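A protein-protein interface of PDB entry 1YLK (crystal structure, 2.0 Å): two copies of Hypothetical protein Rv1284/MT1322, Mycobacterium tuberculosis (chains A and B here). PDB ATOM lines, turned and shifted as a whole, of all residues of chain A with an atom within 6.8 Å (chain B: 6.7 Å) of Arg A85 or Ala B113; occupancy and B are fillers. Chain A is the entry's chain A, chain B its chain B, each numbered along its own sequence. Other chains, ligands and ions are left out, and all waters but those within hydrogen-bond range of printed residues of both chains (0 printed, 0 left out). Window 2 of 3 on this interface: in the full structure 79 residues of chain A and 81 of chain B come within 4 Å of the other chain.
The backbone carbonyl oxygen (O) of Ile A82 is in hydrogen-bond range of the backbone NH (N) of Leu A87 (3.4 Å).
O of Ile B114 sits at hydrogen-bond distance from OG1 of Thr B118 (2.9 Å).
The side-chain hydroxyl (OG1) of Thr B118 lies within hydrogen-bond range of the backbone carbonyl oxygen (O) of Ile B120 (3.0 Å).
No position is printed for both chains.
NH1 of Arg A85 is in salt-bridge range of OE2 of Glu B117, 2.8 Å away.
Of the 12 printed residues of chain B, 5 touch a printed residue of chain A.
Hydrophobic or aromatic side chains of chain B within 4 Å of the printed part of chain A: Phe B110, Ala B113, Ile B114 and Ile B120.
Hydrophobic or aromatic side chains of chain A that line the printed part of chain B: Ile A82, Leu A86 and Phe A148.
Among the printed residues, merely in contact across the chains: Phe A148 with Ile B114, Arg A85 with Ile B114, Arg A85 with Ala B113, Leu A86 with Phe B110, Phe A148 with Ile B120, Ile A82 with Phe B110 and Ala A81 with Phe B110.
Arg A85 touches three residues of chain B.
Of the printed residues of chain A, Ala B113 touches Arg A85 (3.6 Å).
Of the printed residues of chain A, Glu B117 touches Arg A85.
Of the printed residues of chain A, Ile B114 touches Arg A85 (3.5 Å) and Phe A148 (3.4 Å).
Of the printed residues of chain B, Leu A86 touches Phe B110 (3.6 Å).
Lys A151 touches none of the printed residues of chain B.
The nearest printed residue of chain A that does not touch Ala B113 is Leu A86 (7.1 Å).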
ATOM      1  N   LEU A  80     -17.226 -20.002   4.581  1.00  0.00           N
ATOM      2  CA  LEU A  80     -16.596 -20.217   5.889  1.00  0.00           C
ATOM      3  C   LEU A  80     -15.840 -18.974   6.378  1.00  0.00           C
ATOM      4  O   LEU A  80     -15.804 -18.686   7.592  1.00  0.00           O
ATOM      5  CB  LEU A  80     -15.646 -21.416   5.819  1.00  0.00           C
ATOM      6  CG  LEU A  80     -16.259 -22.811   5.712  1.00  0.00           C
ATOM      7  CD1 LEU A  80     -15.131 -23.797   5.380  1.00  0.00           C
ATOM      8  CD2 LEU A  80     -16.981 -23.196   7.021  1.00  0.00           C
ATOM      9  N   ALA A  81     -15.238 -18.242   5.443  1.00  0.00           N
ATOM     10  CA  ALA A  81     -14.526 -17.016   5.779  1.00  0.00           C
ATOM     11  C   ALA A  81     -15.521 -15.995   6.316  1.00  0.00           C
ATOM     12  O   ALA A  81     -15.274 -15.393   7.359  1.00  0.00           O
ATOM     13  CB  ALA A  81     -13.739 -16.469   4.572  1.00  0.00           C
ATOM     14  N   ILE A  82     -16.658 -15.821   5.629  1.00  0.00           N
ATOM     15  CA  ILE A  82     -17.716 -14.930   6.117  1.00  0.00           C
ATOM     16  C   ILE A  82     -18.212 -15.436   7.471  1.00  0.00           C
ATOM     17  O   ILE A  82     -18.320 -14.669   8.432  1.00  0.00           O
ATOM     18  CB  ILE A  82     -18.899 -14.803   5.124  1.00  0.00           C
ATOM     19  CG1 ILE A  82     -18.478 -13.980   3.903  1.00  0.00           C
ATOM     20  CG2 ILE A  82     -20.106 -14.111   5.796  1.00  0.00           C
ATOM     21  CD1 ILE A  82     -19.372 -14.206   2.697  1.00  0.00           C
ATOM     22  N   SER A  83     -18.488 -16.740   7.532  1.00  0.00           N
ATOM     23  CA  SER A  83     -18.940 -17.390   8.767  1.00  0.00           C
ATOM     24  C   SER A  83     -18.039 -17.080   9.968  1.00  0.00           C
ATOM     25  O   SER A  83     -18.535 -16.710  11.038  1.00  0.00           O
ATOM     26  CB  SER A  83     -19.077 -18.905   8.568  1.00  0.00           C
ATOM     27  OG  SER A  83     -19.541 -19.522   9.767  1.00  0.00           O
ATOM     28  N   GLN A  84     -16.731 -17.242   9.798  1.00  0.00           N
ATOM     29  CA  GLN A  84     -15.780 -17.026  10.893  1.00  0.00           C
ATOM     30  C   GLN A  84     -15.501 -15.552  11.166  1.00  0.00           C
ATOM     31  O   GLN A  84     -15.584 -15.098  12.322  1.00  0.00           O
ATOM     32  CB  GLN A  84     -14.457 -17.753  10.620  1.00  0.00           C
ATOM     33  CG  GLN A  84     -14.568 -19.250  10.529  1.00  0.00           C
ATOM     34  CD  GLN A  84     -13.205 -19.930  10.413  1.00  0.00           C
ATOM     35  OE1 GLN A  84     -12.206 -19.303  10.043  1.00  0.00           O
ATOM     36  NE2 GLN A  84     -13.161 -21.211  10.749  1.00  0.00           N
ATOM     37  N   ARG A  85     -15.175 -14.800  10.116  1.00  0.00           N
ATOM     38  CA  ARG A  85     -14.724 -13.410  10.275  1.00  0.00           C
ATOM     39  C   ARG A  85     -15.842 -12.434  10.605  1.00  0.00           C
ATOM     40  O   ARG A  85     -15.640 -11.510  11.385  1.00  0.00           O
ATOM     41  CB  ARG A  85     -14.010 -12.915   9.019  1.00  0.00           C
ATOM     42  CG  ARG A  85     -12.766 -13.722   8.645  1.00  0.00           C
ATOM     43  CD  ARG A  85     -12.038 -13.060   7.492  1.00  0.00           C
ATOM     44  NE  ARG A  85     -11.752 -11.654   7.786  1.00  0.00           N
ATOM     45  CZ  ARG A  85     -10.672 -11.229   8.435  1.00  0.00           C
ATOM     46  NH1 ARG A  85      -9.757 -12.097   8.863  1.00  0.00           N
ATOM     47  NH2 ARG A  85     -10.502  -9.935   8.650  1.00  0.00           N
ATOM     48  N   LEU A  86     -17.016 -12.620  10.006  1.00  0.00           N
ATOM     49  CA  LEU A  86     -18.111 -11.679  10.249  1.00  0.00           C
ATOM     50  C   LEU A  86     -19.099 -12.152  11.303  1.00  0.00           C
ATOM     51  O   LEU A  86     -19.742 -11.342  11.968  1.00  0.00           O
ATOM     52  CB  LEU A  86     -18.837 -11.334   8.943  1.00  0.00           C
ATOM     53  CG  LEU A  86     -17.964 -10.642   7.883  1.00  0.00           C
ATOM     54  CD1 LEU A  86     -18.803 -10.312   6.682  1.00  0.00           C
ATOM     55  CD2 LEU A  86     -17.262  -9.364   8.414  1.00  0.00           C
ATOM     56  N   LEU A  87     -19.214 -13.467  11.452  1.00  0.00           N
ATOM     57  CA  LEU A  87     -20.286 -14.055  12.252  1.00  0.00           C
ATOM     58  C   LEU A  87     -19.814 -14.979  13.379  1.00  0.00           C
ATOM     59  O   LEU A  87     -20.630 -15.688  13.963  1.00  0.00           O
ATOM     60  CB  LEU A  87     -21.305 -14.760  11.338  1.00  0.00           C
ATOM     61  CG  LEU A  87     -22.015 -13.746  10.418  1.00  0.00           C
ATOM     62  CD1 LEU A  87     -22.748 -14.449   9.320  1.00  0.00           C
ATOM     63  CD2 LEU A  87     -22.937 -12.775  11.170  1.00  0.00           C
ATOM     64  N   GLY A  88     -18.504 -14.959  13.659  1.00  0.00           N
ATOM     65  CA  GLY A  88     -17.919 -15.510  14.897  1.00  0.00           C
ATOM     66  C   GLY A  88     -17.908 -17.034  15.053  1.00  0.00           C
ATOM     67  O   GLY A  88     -17.801 -17.537  16.165  1.00  0.00           O
ATOM     68  N   THR A  89     -18.019 -17.786  13.966  1.00  0.00           N
ATOM     69  CA  THR A  89     -17.935 -19.251  14.100  1.00  0.00           C
ATOM     70  C   THR A  89     -16.476 -19.690  14.291  1.00  0.00           C
ATOM     71  O   THR A  89     -15.560 -19.041  13.784  1.00  0.00           O
ATOM     72  CB  THR A  89     -18.637 -20.001  12.955  1.00  0.00           C
ATOM     73  OG1 THR A  89     -17.895 -19.837  11.732  1.00  0.00           O
ATOM     74  CG2 THR A  89     -20.079 -19.501  12.793  1.00  0.00           C
ATOM     75  N   PHE A 148      -7.395 -18.336   4.521  1.00  0.00           N
ATOM     76  CA  PHE A 148      -8.563 -17.485   4.807  1.00  0.00           C
ATOM     77  C   PHE A 148      -9.522 -18.038   5.853  1.00  0.00           C
ATOM     78  O   PHE A 148     -10.449 -17.343   6.273  1.00  0.00           O
ATOM     79  CB  PHE A 148      -9.328 -17.182   3.508  1.00  0.00           C
ATOM     80  CG  PHE A 148      -8.456 -16.626   2.406  1.00  0.00           C
ATOM     81  CD1 PHE A 148      -8.448 -17.206   1.141  1.00  0.00           C
ATOM     82  CD2 PHE A 148      -7.629 -15.527   2.645  1.00  0.00           C
ATOM     83  CE1 PHE A 148      -7.635 -16.695   0.138  1.00  0.00           C
ATOM     84  CE2 PHE A 148      -6.809 -15.015   1.640  1.00  0.00           C
ATOM     85  CZ  PHE A 148      -6.820 -15.602   0.390  1.00  0.00           C
ATOM     86  N   THR A 150      -8.993 -19.674   9.205  1.00  0.00           N
ATOM     87  CA  THR A 150      -7.980 -20.047  10.191  1.00  0.00           C
ATOM     88  C   THR A 150      -8.466 -19.874  11.624  1.00  0.00           C
ATOM     89  O   THR A 150      -7.743 -20.215  12.564  1.00  0.00           O
ATOM     90  CB  THR A 150      -6.658 -19.260   9.982  1.00  0.00           C
ATOM     91  OG1 THR A 150      -6.932 -17.855   9.988  1.00  0.00           O
ATOM     92  CG2 THR A 150      -6.001 -19.646   8.650  1.00  0.00           C
ATOM     93  N   LYS A 151      -9.697 -19.373  11.786  1.00  0.00           N
ATOM     94  CA  LYS A 151     -10.210 -18.977  13.110  1.00  0.00           C
ATOM     95  C   LYS A 151     -10.832 -20.128  13.907  1.00  0.00           C
ATOM     96  O   LYS A 151     -11.288 -19.930  15.036  1.00  0.00           O
ATOM     97  CB  LYS A 151     -11.201 -17.802  12.995  1.00  0.00           C
ATOM     98  CG  LYS A 151     -10.549 -16.469  12.604  1.00  0.00           C
ATOM     99  CD  LYS A 151     -11.549 -15.307  12.646  1.00  0.00           C
ATOM    100  CE  LYS A 151     -10.843 -13.958  12.869  1.00  0.00           C
ATOM    101  NZ  LYS A 151     -11.809 -12.807  13.035  1.00  0.00           N
ATOM    102  N   ASP B 108     -15.082  -5.007  -1.186  1.00  0.00           N
ATOM    103  CA  ASP B 108     -13.796  -4.322  -1.059  1.00  0.00           C
ATOM    104  C   ASP B 108     -13.280  -4.245   0.382  1.00  0.00           C
ATOM    105  O   ASP B 108     -12.112  -4.549   0.633  1.00  0.00           O
ATOM    106  CB  ASP B 108     -13.854  -2.915  -1.683  1.00  0.00           C
ATOM    107  CG  ASP B 108     -13.989  -2.939  -3.205  1.00  0.00           C
ATOM    108  OD1 ASP B 108     -13.561  -3.925  -3.845  1.00  0.00           O
ATOM    109  OD2 ASP B 108     -14.521  -1.955  -3.773  1.00  0.00           O
ATOM    110  N   ASP B 109     -14.151  -3.869   1.321  1.00  0.00           N
ATOM    111  CA  ASP B 109     -13.768  -3.747   2.739  1.00  0.00           C
ATOM    112  C   ASP B 109     -13.387  -5.111   3.301  1.00  0.00           C
ATOM    113  O   ASP B 109     -12.411  -5.229   4.039  1.00  0.00           O
ATOM    114  CB  ASP B 109     -14.912  -3.175   3.587  1.00  0.00           C
ATOM    115  CG  ASP B 109     -15.161  -1.679   3.357  1.00  0.00           C
ATOM    116  OD1 ASP B 109     -14.323  -0.963   2.747  1.00  0.00           O
ATOM    117  OD2 ASP B 109     -16.231  -1.217   3.809  1.00  0.00           O
ATOM    118  N   PHE B 110     -14.167  -6.136   2.943  1.00  0.00           N
ATOM    119  CA  PHE B 110     -13.949  -7.511   3.411  1.00  0.00           C
ATOM    120  C   PHE B 110     -12.601  -8.031   2.919  1.00  0.00           C
ATOM    121  O   PHE B 110     -11.854  -8.639   3.682  1.00  0.00           O
ATOM    122  CB  PHE B 110     -15.092  -8.435   2.929  1.00  0.00           C
ATOM    123  CG  PHE B 110     -15.058  -9.834   3.522  1.00  0.00           C
ATOM    124  CD1 PHE B 110     -15.398 -10.054   4.852  1.00  0.00           C
ATOM    125  CD2 PHE B 110     -14.720 -10.930   2.741  1.00  0.00           C
ATOM    126  CE1 PHE B 110     -15.385 -11.345   5.400  1.00  0.00           C
ATOM    127  CE2 PHE B 110     -14.711 -12.218   3.277  1.00  0.00           C
ATOM    128  CZ  PHE B 110     -15.039 -12.421   4.613  1.00  0.00           C
ATOM    129  N   LYS B 111     -12.306  -7.800   1.641  1.00  0.00           N
ATOM    130  CA  LYS B 111     -11.041  -8.233   1.050  1.00  0.00           C
ATOM    131  C   LYS B 111      -9.861  -7.491   1.647  1.00  0.00           C
ATOM    132  O   LYS B 111      -8.824  -8.094   1.912  1.00  0.00           O
ATOM    133  CB  LYS B 111     -11.039  -8.076  -0.477  1.00  0.00           C
ATOM    134  CG  LYS B 111     -11.750  -9.218  -1.183  1.00  0.00           C
ATOM    135  CD  LYS B 111     -11.209  -9.408  -2.593  1.00  0.00           C
ATOM    136  CE  LYS B 111     -12.142 -10.279  -3.385  1.00  0.00           C
ATOM    137  NZ  LYS B 111     -11.597 -10.660  -4.699  1.00  0.00           N
ATOM    138  N   ARG B 112     -10.037  -6.186   1.874  1.00  0.00           N
ATOM    139  CA  ARG B 112      -9.007  -5.358   2.494  1.00  0.00           C
ATOM    140  C   ARG B 112      -8.630  -5.871   3.887  1.00  0.00           C
ATOM    141  O   ARG B 112      -7.448  -6.003   4.199  1.00  0.00           O
ATOM    142  CB  ARG B 112      -9.473  -3.897   2.569  1.00  0.00           C
ATOM    143  CG  ARG B 112      -8.361  -2.868   2.481  1.00  0.00           C
ATOM    144  CD  ARG B 112      -8.934  -1.460   2.225  1.00  0.00           C
ATOM    145  NE  ARG B 112     -10.180  -1.518   1.457  1.00  0.00           N
ATOM    146  CZ  ARG B 112     -10.766  -0.485   0.859  1.00  0.00           C
ATOM    147  NH1 ARG B 112     -10.220   0.727   0.915  1.00  0.00           N
ATOM    148  NH2 ARG B 112     -11.901  -0.675   0.192  1.00  0.00           N
ATOM    149  N   ALA B 113      -9.641  -6.178   4.700  1.00  0.00           N
ATOM    150  CA  ALA B 113      -9.458  -6.676   6.071  1.00  0.00           C
ATOM    151  C   ALA B 113      -8.733  -8.027   6.093  1.00  0.00           C
ATOM    152  O   ALA B 113      -7.852  -8.271   6.921  1.00  0.00           O
ATOM    153  CB  ALA B 113     -10.821  -6.792   6.770  1.00  0.00           C
ATOM    154  N   ILE B 114      -9.113  -8.897   5.167  1.00  0.00           N
ATOM    155  CA  ILE B 114      -8.466 -10.195   4.998  1.00  0.00           C
ATOM    156  C   ILE B 114      -7.006  -9.997   4.608  1.00  0.00           C
ATOM    157  O   ILE B 114      -6.121 -10.635   5.172  1.00  0.00           O
ATOM    158  CB  ILE B 114      -9.215 -11.068   3.956  1.00  0.00           C
ATOM    159  CG1 ILE B 114     -10.565 -11.500   4.516  1.00  0.00           C
ATOM    160  CG2 ILE B 114      -8.386 -12.298   3.582  1.00  0.00           C
ATOM    161  CD1 ILE B 114     -11.256 -12.583   3.708  1.00  0.00           C
ATOM    162  N   GLN B 115      -6.754  -9.096   3.661  1.00  0.00           N
ATOM    163  CA  GLN B 115      -5.386  -8.833   3.225  1.00  0.00           C
ATOM    164  C   GLN B 115      -4.559  -8.220   4.360  1.00  0.00           C
ATOM    165  O   GLN B 115      -3.404  -8.605   4.578  1.00  0.00           O
ATOM    166  CB  GLN B 115      -5.364  -7.936   1.982  1.00  0.00           C
ATOM    167  CG  GLN B 115      -3.953  -7.594   1.485  1.00  0.00           C
ATOM    168  CD  GLN B 115      -3.947  -6.798   0.205  1.00  0.00           C
ATOM    169  OE1 GLN B 115      -4.992  -6.536  -0.389  1.00  0.00           O
ATOM    170  NE2 GLN B 115      -2.762  -6.395  -0.226  1.00  0.00           N
ATOM    171  N   ASP B 116      -5.162  -7.279   5.084  1.00  0.00           N
ATOM    172  CA  ASP B 116      -4.507  -6.621   6.225  1.00  0.00           C
ATOM    173  C   ASP B 116      -3.961  -7.657   7.198  1.00  0.00           C
ATOM    174  O   ASP B 116      -2.824  -7.556   7.671  1.00  0.00           O
ATOM    175  CB  ASP B 116      -5.482  -5.683   6.944  1.00  0.00           C
ATOM    176  CG  ASP B 116      -5.635  -4.337   6.243  1.00  0.00           C
ATOM    177  OD1 ASP B 116      -4.896  -4.078   5.261  1.00  0.00           O
ATOM    178  OD2 ASP B 116      -6.498  -3.530   6.682  1.00  0.00           O
ATOM    179  N   GLU B 117      -4.772  -8.675   7.457  1.00  0.00           N
ATOM    180  CA  GLU B 117      -4.451  -9.659   8.466  1.00  0.00           C
ATOM    181  C   GLU B 117      -3.618 -10.820   7.921  1.00  0.00           C
ATOM    182  O   GLU B 117      -2.717 -11.284   8.613  1.00  0.00           O
ATOM    183  CB  GLU B 117      -5.740 -10.136   9.127  1.00  0.00           C
ATOM    184  CG  GLU B 117      -5.584 -11.304  10.085  1.00  0.00           C
ATOM    185  CD  GLU B 117      -6.906 -11.975  10.362  1.00  0.00           C
ATOM    186  OE1 GLU B 117      -6.976 -13.215  10.223  1.00  0.00           O
ATOM    187  OE2 GLU B 117      -7.877 -11.259  10.696  1.00  0.00           O
ATOM    188  N   THR B 118      -3.903 -11.282   6.698  1.00  0.00           N
ATOM    189  CA  THR B 118      -3.175 -12.433   6.112  1.00  0.00           C
ATOM    190  C   THR B 118      -2.015 -12.099   5.162  1.00  0.00           C
ATOM    191  O   THR B 118      -1.170 -12.950   4.909  1.00  0.00           O
ATOM    192  CB  THR B 118      -4.100 -13.409   5.367  1.00  0.00           C
ATOM    193  OG1 THR B 118      -4.557 -12.809   4.146  1.00  0.00           O
ATOM    194  CG2 THR B 118      -5.279 -13.817   6.233  1.00  0.00           C
ATOM    195  N   ILE B 120      -2.663 -11.544   2.122  1.00  0.00           N
ATOM    196  CA  ILE B 120      -3.190 -12.059   0.851  1.00  0.00           C
ATOM    197  C   ILE B 120      -4.635 -11.601   0.617  1.00  0.00           C
ATOM    198  O   ILE B 120      -5.441 -11.594   1.550  1.00  0.00           O
ATOM    199  CB  ILE B 120      -3.082 -13.614   0.793  1.00  0.00           C
ATOM    200  CG1 ILE B 120      -1.633 -14.073   1.048  1.00  0.00           C
ATOM    201  CG2 ILE B 120      -3.577 -14.155  -0.561  1.00  0.00           C
ATOM    202  CD1 ILE B 120      -1.496 -15.492   1.614  1.00  0.00           C
